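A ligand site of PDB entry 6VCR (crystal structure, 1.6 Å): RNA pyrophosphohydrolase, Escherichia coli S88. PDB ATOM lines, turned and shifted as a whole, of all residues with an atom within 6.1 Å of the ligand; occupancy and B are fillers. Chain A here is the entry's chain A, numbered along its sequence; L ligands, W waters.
NE2 of Gln 38 touches O6 of the ligand (3.6 Å).
CD2 of Leu 80 touches C9 of the ligand, 3.6 Å away.
CD1 of Leu 84 touches O3 of the ligand (3.8 Å).
CB of Val 138 touches N3 of the ligand (3.8 Å).
CZ of Phe 140 touches C4 of the ligand (3.9 Å).
Hydrophobic or aromatic side chains within 4 Å of the ligand: Tyr 78, Leu 80, Leu 84, Val 138 and Phe 140.
11 residues have an atom within 4 Å of the ligand: Arg 28, Gln 31, Ser 33, Gln 38, Tyr 78, Leu 80, Leu 84, Gln 96, Val 138, Phe 140 and Lys 141.
Water W10 bridges an oxygen (O14) of the ligand and the backbone NH (N) of Gly 40.
Water W6 bridges O13 of the ligand (2.7 Å) and OD1 of Asn 11 (2.9 Å).
Water W5 lies within hydrogen-bond range of O14 of the ligand, OD1 of Asn 11, NE2 of Gln 38 and NE2 of Gln 96.
Water W2 bridges the side-chain amide nitrogen (NE2) of Gln 96 and an oxygen (O7) of the ligand.
Water W11 bridges the backbone carbonyl oxygen of Gln 38 (2.7 Å) and an oxygen (O14) of the ligand (2.9 Å).
Water W8 lies within hydrogen-bond range of OE1 of Gln 35, NZ of Lys 141 and N3 of the ligand.
OG of Ser 33 sits at hydrogen-bond distance from N3 of the ligand (3.0 Å).
The side-chain amino group (NZ) of Lys 141 is in salt-bridge range of an oxygen (O6) of the ligand, at 2.6 Å.
O7 of the ligand lies within hydrogen-bond range of OH of Tyr 78 (2.6 Å).
The side-chain amide nitrogen (NE2) of Gln 31 sits at hydrogen-bond distance from a nitrogen (N2) of the ligand.
NH1 of Arg 28 lies within salt-bridge range of O9 of the ligand (2.9 Å).
NE2 of Gln 96 is in hydrogen-bond range of O7 of the ligand (3.3 Å).
N of Arg 28 is in hydrogen-bond range of O of Ser 33 (2.9 Å).
The side-chain amide oxygen (OE1) of Gln 96 sits close to the side-chain amide nitrogen (ND2) of Asn 11 (3.1 Å).
NH2 of Arg 28 is in hydrogen-bond range of OE1 of Gln 35, 2.9 Å away.
The side-chain amino group (NZ) of Lys 141 is in hydrogen-bond range of the side-chain amide oxygen (OE1) of Gln 35 (3.1 Å).
OE1 of Gln 96 sits at hydrogen-bond distance from NE2 of Gln 38, 3.1 Å away.
O of Gln 96 is in hydrogen-bond range of N of Tyr 78 (3.1 Å).
The side-chain amino group (NZ) of Lys 141 is in hydrogen-bond range of the side-chain amide oxygen (OE1) of Gln 38 (2.9 Å).
The side-chain hydroxyl (OH) of Tyr 78 lies within hydrogen-bond range of the side-chain amide nitrogen (NE2) of Gln 38 (3.0 Å).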
ATOM      1  N   ARG A   9      12.509 -12.516  -2.602  1.00  0.00           N
ATOM      2  CA  ARG A   9      11.066 -12.350  -2.754  1.00  0.00           C
ATOM      3  C   ARG A   9      10.387 -12.466  -1.392  1.00  0.00           C
ATOM      4  O   ARG A   9      10.704 -13.390  -0.630  1.00  0.00           O
ATOM      5  CB  ARG A   9      10.484 -13.406  -3.687  1.00  0.00           C
ATOM      6  CG  ARG A   9      10.746 -13.181  -5.174  1.00  0.00           C
ATOM      7  CD  ARG A   9       9.994 -14.235  -5.981  1.00  0.00           C
ATOM      8  NE  ARG A   9      10.565 -14.474  -7.309  1.00  0.00           N
ATOM      9  CZ  ARG A   9      10.154 -13.865  -8.413  1.00  0.00           C
ATOM     10  NH1 ARG A   9       9.160 -12.988  -8.352  1.00  0.00           N
ATOM     11  NH2 ARG A   9      10.717 -14.139  -9.582  1.00  0.00           N
ATOM     12  N   ASN A  11       7.649 -13.657   1.152  1.00  0.00           N
ATOM     13  CA  ASN A  11       6.839 -14.871   1.173  1.00  0.00           C
ATOM     14  C   ASN A  11       6.337 -15.123   2.583  1.00  0.00           C
ATOM     15  O   ASN A  11       6.884 -14.608   3.552  1.00  0.00           O
ATOM     16  CB  ASN A  11       7.646 -16.080   0.687  1.00  0.00           C
ATOM     17  CG  ASN A  11       7.780 -16.131  -0.827  1.00  0.00           C
ATOM     18  OD1 ASN A  11       7.004 -16.798  -1.508  1.00  0.00           O
ATOM     19  ND2 ASN A  11       8.786 -15.460  -1.367  1.00  0.00           N
ATOM     20  N   ARG A  28       5.812 -31.746  -2.202  1.00  0.00           N
ATOM     21  CA  ARG A  28       5.931 -30.858  -3.353  1.00  0.00           C
ATOM     22  C   ARG A  28       5.475 -31.603  -4.606  1.00  0.00           C
ATOM     23  O   ARG A  28       5.853 -32.762  -4.833  1.00  0.00           O
ATOM     24  CB  ARG A  28       7.379 -30.374  -3.513  1.00  0.00           C
ATOM     25  CG  ARG A  28       7.821 -29.318  -2.486  1.00  0.00           C
ATOM     26  CD  ARG A  28       9.284 -28.944  -2.712  1.00  0.00           C
ATOM     27  NE  ARG A  28       9.464 -28.297  -4.011  1.00  0.00           N
ATOM     28  CZ  ARG A  28       9.402 -26.980  -4.216  1.00  0.00           C
ATOM     29  NH1 ARG A  28       9.586 -26.489  -5.433  1.00  0.00           N
ATOM     30  NH2 ARG A  28       9.167 -26.151  -3.212  1.00  0.00           N
ATOM     31  N   GLN A  31       7.379 -34.374  -6.801  1.00  0.00           N
ATOM     32  CA  GLN A  31       8.668 -34.662  -6.179  1.00  0.00           C
ATOM     33  C   GLN A  31       8.474 -35.655  -5.031  1.00  0.00           C
ATOM     34  O   GLN A  31       7.357 -36.076  -4.723  1.00  0.00           O
ATOM     35  CB  GLN A  31       9.315 -33.375  -5.656  1.00  0.00           C
ATOM     36  CG  GLN A  31       9.554 -32.307  -6.726  1.00  0.00           C
ATOM     37  CD  GLN A  31      10.314 -31.092  -6.193  1.00  0.00           C
ATOM     38  OE1 GLN A  31       9.751 -30.007  -6.084  1.00  0.00           O
ATOM     39  NE2 GLN A  31      11.596 -31.285  -5.874  1.00  0.00           N
ATOM     40  N   SER A  33      10.069 -34.594  -2.149  1.00  0.00           N
ATOM     41  CA  SER A  33      10.560 -33.606  -1.200  1.00  0.00           C
ATOM     42  C   SER A  33       9.346 -32.891  -0.604  1.00  0.00           C
ATOM     43  O   SER A  33       8.427 -32.537  -1.335  1.00  0.00           O
ATOM     44  CB  SER A  33      11.496 -32.620  -1.917  1.00  0.00           C
ATOM     45  OG  SER A  33      12.200 -31.810  -0.975  1.00  0.00           O
ATOM     46  N   TRP A  34       9.340 -32.748   0.709  1.00  0.00           N
ATOM     47  CA  TRP A  34       8.184 -32.278   1.443  1.00  0.00           C
ATOM     48  C   TRP A  34       8.481 -30.959   2.138  1.00  0.00           C
ATOM     49  O   TRP A  34       9.637 -30.648   2.467  1.00  0.00           O
ATOM     50  CB  TRP A  34       7.761 -33.316   2.486  1.00  0.00           C
ATOM     51  CG  TRP A  34       7.321 -34.646   1.912  1.00  0.00           C
ATOM     52  CD1 TRP A  34       8.068 -35.516   1.182  1.00  0.00           C
ATOM     53  CD2 TRP A  34       6.021 -35.264   2.064  1.00  0.00           C
ATOM     54  NE1 TRP A  34       7.323 -36.625   0.855  1.00  0.00           N
ATOM     55  CE2 TRP A  34       6.070 -36.503   1.389  1.00  0.00           C
ATOM     56  CE3 TRP A  34       4.839 -34.894   2.713  1.00  0.00           C
ATOM     57  CZ2 TRP A  34       4.967 -37.354   1.310  1.00  0.00           C
ATOM     58  CZ3 TRP A  34       3.755 -35.749   2.648  1.00  0.00           C
ATOM     59  CH2 TRP A  34       3.836 -36.969   1.951  1.00  0.00           C
ATOM     60  N   GLN A  35       7.426 -30.195   2.413  1.00  0.00           N
ATOM     61  CA  GLN A  35       7.592 -28.893   3.048  1.00  0.00           C
ATOM     62  C   GLN A  35       6.248 -28.423   3.587  1.00  0.00           C
ATOM     63  O   GLN A  35       5.208 -29.024   3.345  1.00  0.00           O
ATOM     64  CB  GLN A  35       8.158 -27.866   2.046  1.00  0.00           C
ATOM     65  CG  GLN A  35       7.139 -27.485   0.987  1.00  0.00           C
ATOM     66  CD  GLN A  35       7.634 -26.458   0.011  1.00  0.00           C
ATOM     67  OE1 GLN A  35       8.813 -26.415  -0.322  1.00  0.00           O
ATOM     68  NE2 GLN A  35       6.728 -25.602  -0.485  1.00  0.00           N
ATOM     69  N   GLN A  38       3.981 -22.512   1.506  1.00  0.00           N
ATOM     70  CA  GLN A  38       4.573 -21.195   1.465  1.00  0.00           C
ATOM     71  C   GLN A  38       4.152 -20.504   0.171  1.00  0.00           C
ATOM     72  O   GLN A  38       3.993 -21.155  -0.876  1.00  0.00           O
ATOM     73  CB  GLN A  38       6.109 -21.250   1.584  1.00  0.00           C
ATOM     74  CG  GLN A  38       6.824 -22.054   0.554  1.00  0.00           C
ATOM     75  CD  GLN A  38       8.322 -21.892   0.659  1.00  0.00           C
ATOM     76  OE1 GLN A  38       8.974 -22.450   1.542  1.00  0.00           O
ATOM     77  NE2 GLN A  38       8.879 -21.108  -0.239  1.00  0.00           N
ATOM     78  N   GLY A  39       3.970 -19.193   0.247  1.00  0.00           N
ATOM     79  CA  GLY A  39       3.570 -18.445  -0.937  1.00  0.00           C
ATOM     80  C   GLY A  39       3.971 -16.996  -0.876  1.00  0.00           C
ATOM     81  O   GLY A  39       4.319 -16.457   0.184  1.00  0.00           O
ATOM     82  N   GLY A  40       3.881 -16.356  -2.020  1.00  0.00           N
ATOM     83  CA  GLY A  40       4.364 -14.997  -2.143  1.00  0.00           C
ATOM     84  C   GLY A  40       3.400 -13.980  -1.573  1.00  0.00           C
ATOM     85  O   GLY A  40       2.204 -14.234  -1.403  1.00  0.00           O
ATOM     86  N   TYR A  78      16.278 -17.423   3.393  1.00  0.00           N
ATOM     87  CA  TYR A  78      17.127 -18.484   2.867  1.00  0.00           C
ATOM     88  C   TYR A  78      17.570 -18.113   1.472  1.00  0.00           C
ATOM     89  O   TYR A  78      16.880 -17.380   0.757  1.00  0.00           O
ATOM     90  CB  TYR A  78      16.457 -19.885   2.843  1.00  0.00           C
ATOM     91  CG  TYR A  78      15.236 -20.065   1.965  1.00  0.00           C
ATOM     92  CD1 TYR A  78      15.338 -20.231   0.590  1.00  0.00           C
ATOM     93  CD2 TYR A  78      13.981 -20.153   2.535  1.00  0.00           C
ATOM     94  CE1 TYR A  78      14.206 -20.428  -0.197  1.00  0.00           C
ATOM     95  CE2 TYR A  78      12.865 -20.334   1.752  1.00  0.00           C
ATOM     96  CZ  TYR A  78      12.976 -20.477   0.401  1.00  0.00           C
ATOM     97  OH  TYR A  78      11.833 -20.677  -0.337  1.00  0.00           O
ATOM     98  N   LEU A  80      18.770 -19.564  -2.301  1.00  0.00           N
ATOM     99  CA  LEU A  80      18.704 -20.732  -3.161  1.00  0.00           C
ATOM    100  C   LEU A  80      20.114 -21.247  -3.432  1.00  0.00           C
ATOM    101  O   LEU A  80      21.050 -20.453  -3.609  1.00  0.00           O
ATOM    102  CB  LEU A  80      18.042 -20.370  -4.481  1.00  0.00           C
ATOM    103  CG  LEU A  80      16.587 -19.897  -4.459  1.00  0.00           C
ATOM    104  CD1 LEU A  80      16.154 -19.520  -5.861  1.00  0.00           C
ATOM    105  CD2 LEU A  80      15.716 -20.987  -3.888  1.00  0.00           C
ATOM    106  N   LEU A  84      20.135 -23.735  -8.566  1.00  0.00           N
ATOM    107  CA  LEU A  84      18.703 -23.566  -8.767  1.00  0.00           C
ATOM    108  C   LEU A  84      18.306 -22.117  -8.985  1.00  0.00           C
ATOM    109  O   LEU A  84      17.106 -21.819  -9.012  1.00  0.00           O
ATOM    110  CB  LEU A  84      17.937 -24.152  -7.592  1.00  0.00           C
ATOM    111  CG  LEU A  84      18.277 -25.588  -7.201  1.00  0.00           C
ATOM    112  CD1 LEU A  84      17.520 -25.954  -5.926  1.00  0.00           C
ATOM    113  CD2 LEU A  84      17.967 -26.574  -8.326  1.00  0.00           C
ATOM    114  N   GLN A  96      14.374 -16.168  -0.661  1.00  0.00           N
ATOM    115  CA  GLN A  96      13.139 -15.657  -0.095  1.00  0.00           C
ATOM    116  C   GLN A  96      13.370 -15.102   1.300  1.00  0.00           C
ATOM    117  O   GLN A  96      14.191 -15.621   2.059  1.00  0.00           O
ATOM    118  CB  GLN A  96      12.062 -16.751   0.009  1.00  0.00           C
ATOM    119  CG  GLN A  96      11.717 -17.443  -1.277  1.00  0.00           C
ATOM    120  CD  GLN A  96      10.404 -18.169  -1.167  1.00  0.00           C
ATOM    121  OE1 GLN A  96       9.751 -18.159  -0.109  1.00  0.00           O
ATOM    122  NE2 GLN A  96       9.983 -18.791  -2.270  1.00  0.00           N
ATOM    123  N   VAL A 138      14.264 -29.776   2.615  1.00  0.00           N
ATOM    124  CA  VAL A 138      15.472 -29.595   1.816  1.00  0.00           C
ATOM    125  C   VAL A 138      16.484 -28.736   2.574  1.00  0.00           C
ATOM    126  O   VAL A 138      16.124 -27.806   3.312  1.00  0.00           O
ATOM    127  CB  VAL A 138      15.102 -29.014   0.443  1.00  0.00           C
ATOM    128  CG1 VAL A 138      14.646 -27.575   0.570  1.00  0.00           C
ATOM    129  CG2 VAL A 138      16.267 -29.136  -0.521  1.00  0.00           C
ATOM    130  N   PHE A 140      18.643 -26.378   2.194  1.00  0.00           N
ATOM    131  CA  PHE A 140      18.810 -24.925   2.245  1.00  0.00           C
ATOM    132  C   PHE A 140      17.679 -24.218   2.991  1.00  0.00           C
ATOM    133  O   PHE A 140      17.785 -23.002   3.227  1.00  0.00           O
ATOM    134  CB  PHE A 140      18.986 -24.340   0.817  1.00  0.00           C
ATOM    135  CG  PHE A 140      17.790 -24.470  -0.092  1.00  0.00           C
ATOM    136  CD1 PHE A 140      16.803 -23.507  -0.116  1.00  0.00           C
ATOM    137  CD2 PHE A 140      17.702 -25.529  -0.989  1.00  0.00           C
ATOM    138  CE1 PHE A 140      15.717 -23.606  -0.989  1.00  0.00           C
ATOM    139  CE2 PHE A 140      16.632 -25.644  -1.860  1.00  0.00           C
ATOM    140  CZ  PHE A 140      15.640 -24.682  -1.864  1.00  0.00           C
ATOM    141  N   LYS A 141      16.648 -24.937   3.431  1.00  0.00           N
ATOM    142  CA  LYS A 141      15.609 -24.319   4.253  1.00  0.00           C
ATOM    143  C   LYS A 141      15.690 -24.715   5.720  1.00  0.00           C
ATOM    144  O   LYS A 141      14.850 -24.278   6.511  1.00  0.00           O
ATOM    145  CB  LYS A 141      14.209 -24.679   3.713  1.00  0.00           C
ATOM    146  CG  LYS A 141      13.951 -24.200   2.305  1.00  0.00           C
ATOM    147  CD  LYS A 141      12.521 -24.496   1.856  1.00  0.00           C
ATOM    148  CE  LYS A 141      12.269 -24.108   0.402  1.00  0.00           C
ATOM    149  NZ  LYS A 141      10.808 -24.112   0.039  1.00  0.00           N
HETATM  150  N1  LIG L   1      13.330 -26.610  -5.531  1.00  0.00           N
HETATM  151  C1  LIG L   1      13.505 -28.047  -5.741  1.00  0.00           C
HETATM  152  N2  LIG L   1      13.291 -28.941  -4.714  1.00  0.00           N
HETATM  153  C2  LIG L   1      12.911 -28.437  -3.519  1.00  0.00           C
HETATM  154  C3  LIG L   1      12.739 -27.062  -3.292  1.00  0.00           C
HETATM  155  C4  LIG L   1      12.960 -26.156  -4.317  1.00  0.00           C
HETATM  156  O1  LIG L   1      13.841 -28.440  -6.794  1.00  0.00           O
HETATM  157  N3  LIG L   1      12.781 -29.337  -2.525  1.00  0.00           N
HETATM  158  C5  LIG L   1      13.583 -25.725  -6.663  1.00  0.00           C
HETATM  159  C6  LIG L   1      12.500 -25.584  -7.477  1.00  0.00           C
HETATM  160  O2  LIG L   1      12.994 -25.543  -8.823  1.00  0.00           O
HETATM  161  C7  LIG L   1      11.844 -24.247  -7.062  1.00  0.00           C
HETATM  162  C8  LIG L   1      13.068 -23.449  -6.622  1.00  0.00           C
HETATM  163  O3  LIG L   1      13.985 -24.468  -6.155  1.00  0.00           O
HETATM  164  O4  LIG L   1      11.175 -23.630  -8.170  1.00  0.00           O
HETATM  165  C9  LIG L   1      12.828 -22.466  -5.473  1.00  0.00           C
HETATM  166  O5  LIG L   1      12.184 -23.214  -4.479  1.00  0.00           O
HETATM  167  P1  LIG L   1      11.288 -22.348  -3.433  1.00  0.00           P
HETATM  168  O6  LIG L   1      10.677 -23.336  -2.469  1.00  0.00           O
HETATM  169  O7  LIG L   1      12.149 -21.250  -2.824  1.00  0.00           O
HETATM  170  O8  LIG L   1      10.152 -21.660  -4.331  1.00  0.00           O
HETATM  171  P2  LIG L   1       9.110 -22.275  -5.385  1.00  0.00           P
HETATM  172  O9  LIG L   1       8.876 -23.741  -5.102  1.00  0.00           O
HETATM  173  O10 LIG L   1       9.616 -22.043  -6.786  1.00  0.00           O
HETATM  174  O11 LIG L   1       7.782 -21.548  -5.132  1.00  0.00           O
HETATM  175  P3  LIG L   1       7.259 -20.073  -5.478  1.00  0.00           P
HETATM  176  O12 LIG L   1       6.660 -20.036  -6.891  1.00  0.00           O
HETATM  177  O13 LIG L   1       8.354 -19.059  -5.338  1.00  0.00           O
HETATM  178  O14 LIG L   1       6.123 -19.786  -4.476  1.00  0.00           O
HETATM  179  O   HOH W   1       7.687 -23.549  -2.260  1.00  0.00           O
HETATM  180  O   HOH W   2      11.603 -19.060  -4.633  1.00  0.00           O
HETATM  181  O   HOH W   3      14.460 -31.671  -3.824  1.00  0.00           O
HETATM  182  O   HOH W   4       6.300 -24.682  -5.522  1.00  0.00           O
HETATM  183  O   HOH W   5       6.960 -19.629  -1.888  1.00  0.00           O
HETATM  184  O   HOH W   6       7.855 -16.694  -4.229  1.00  0.00           O
HETATM  185  O   HOH W   7      14.692 -21.230  -8.741  1.00  0.00           O
HETATM  186  O   HOH W   8      11.249 -27.482  -0.027  1.00  0.00           O
HETATM  187  O   HOH W   9       4.160 -20.842  -7.079  1.00  0.00           O
HETATM  188  O   HOH W  10       4.306 -18.136  -4.581  1.00  0.00           O
HETATM  189  O   HOH W  11       4.973 -22.141  -3.186  1.00  0.00           O
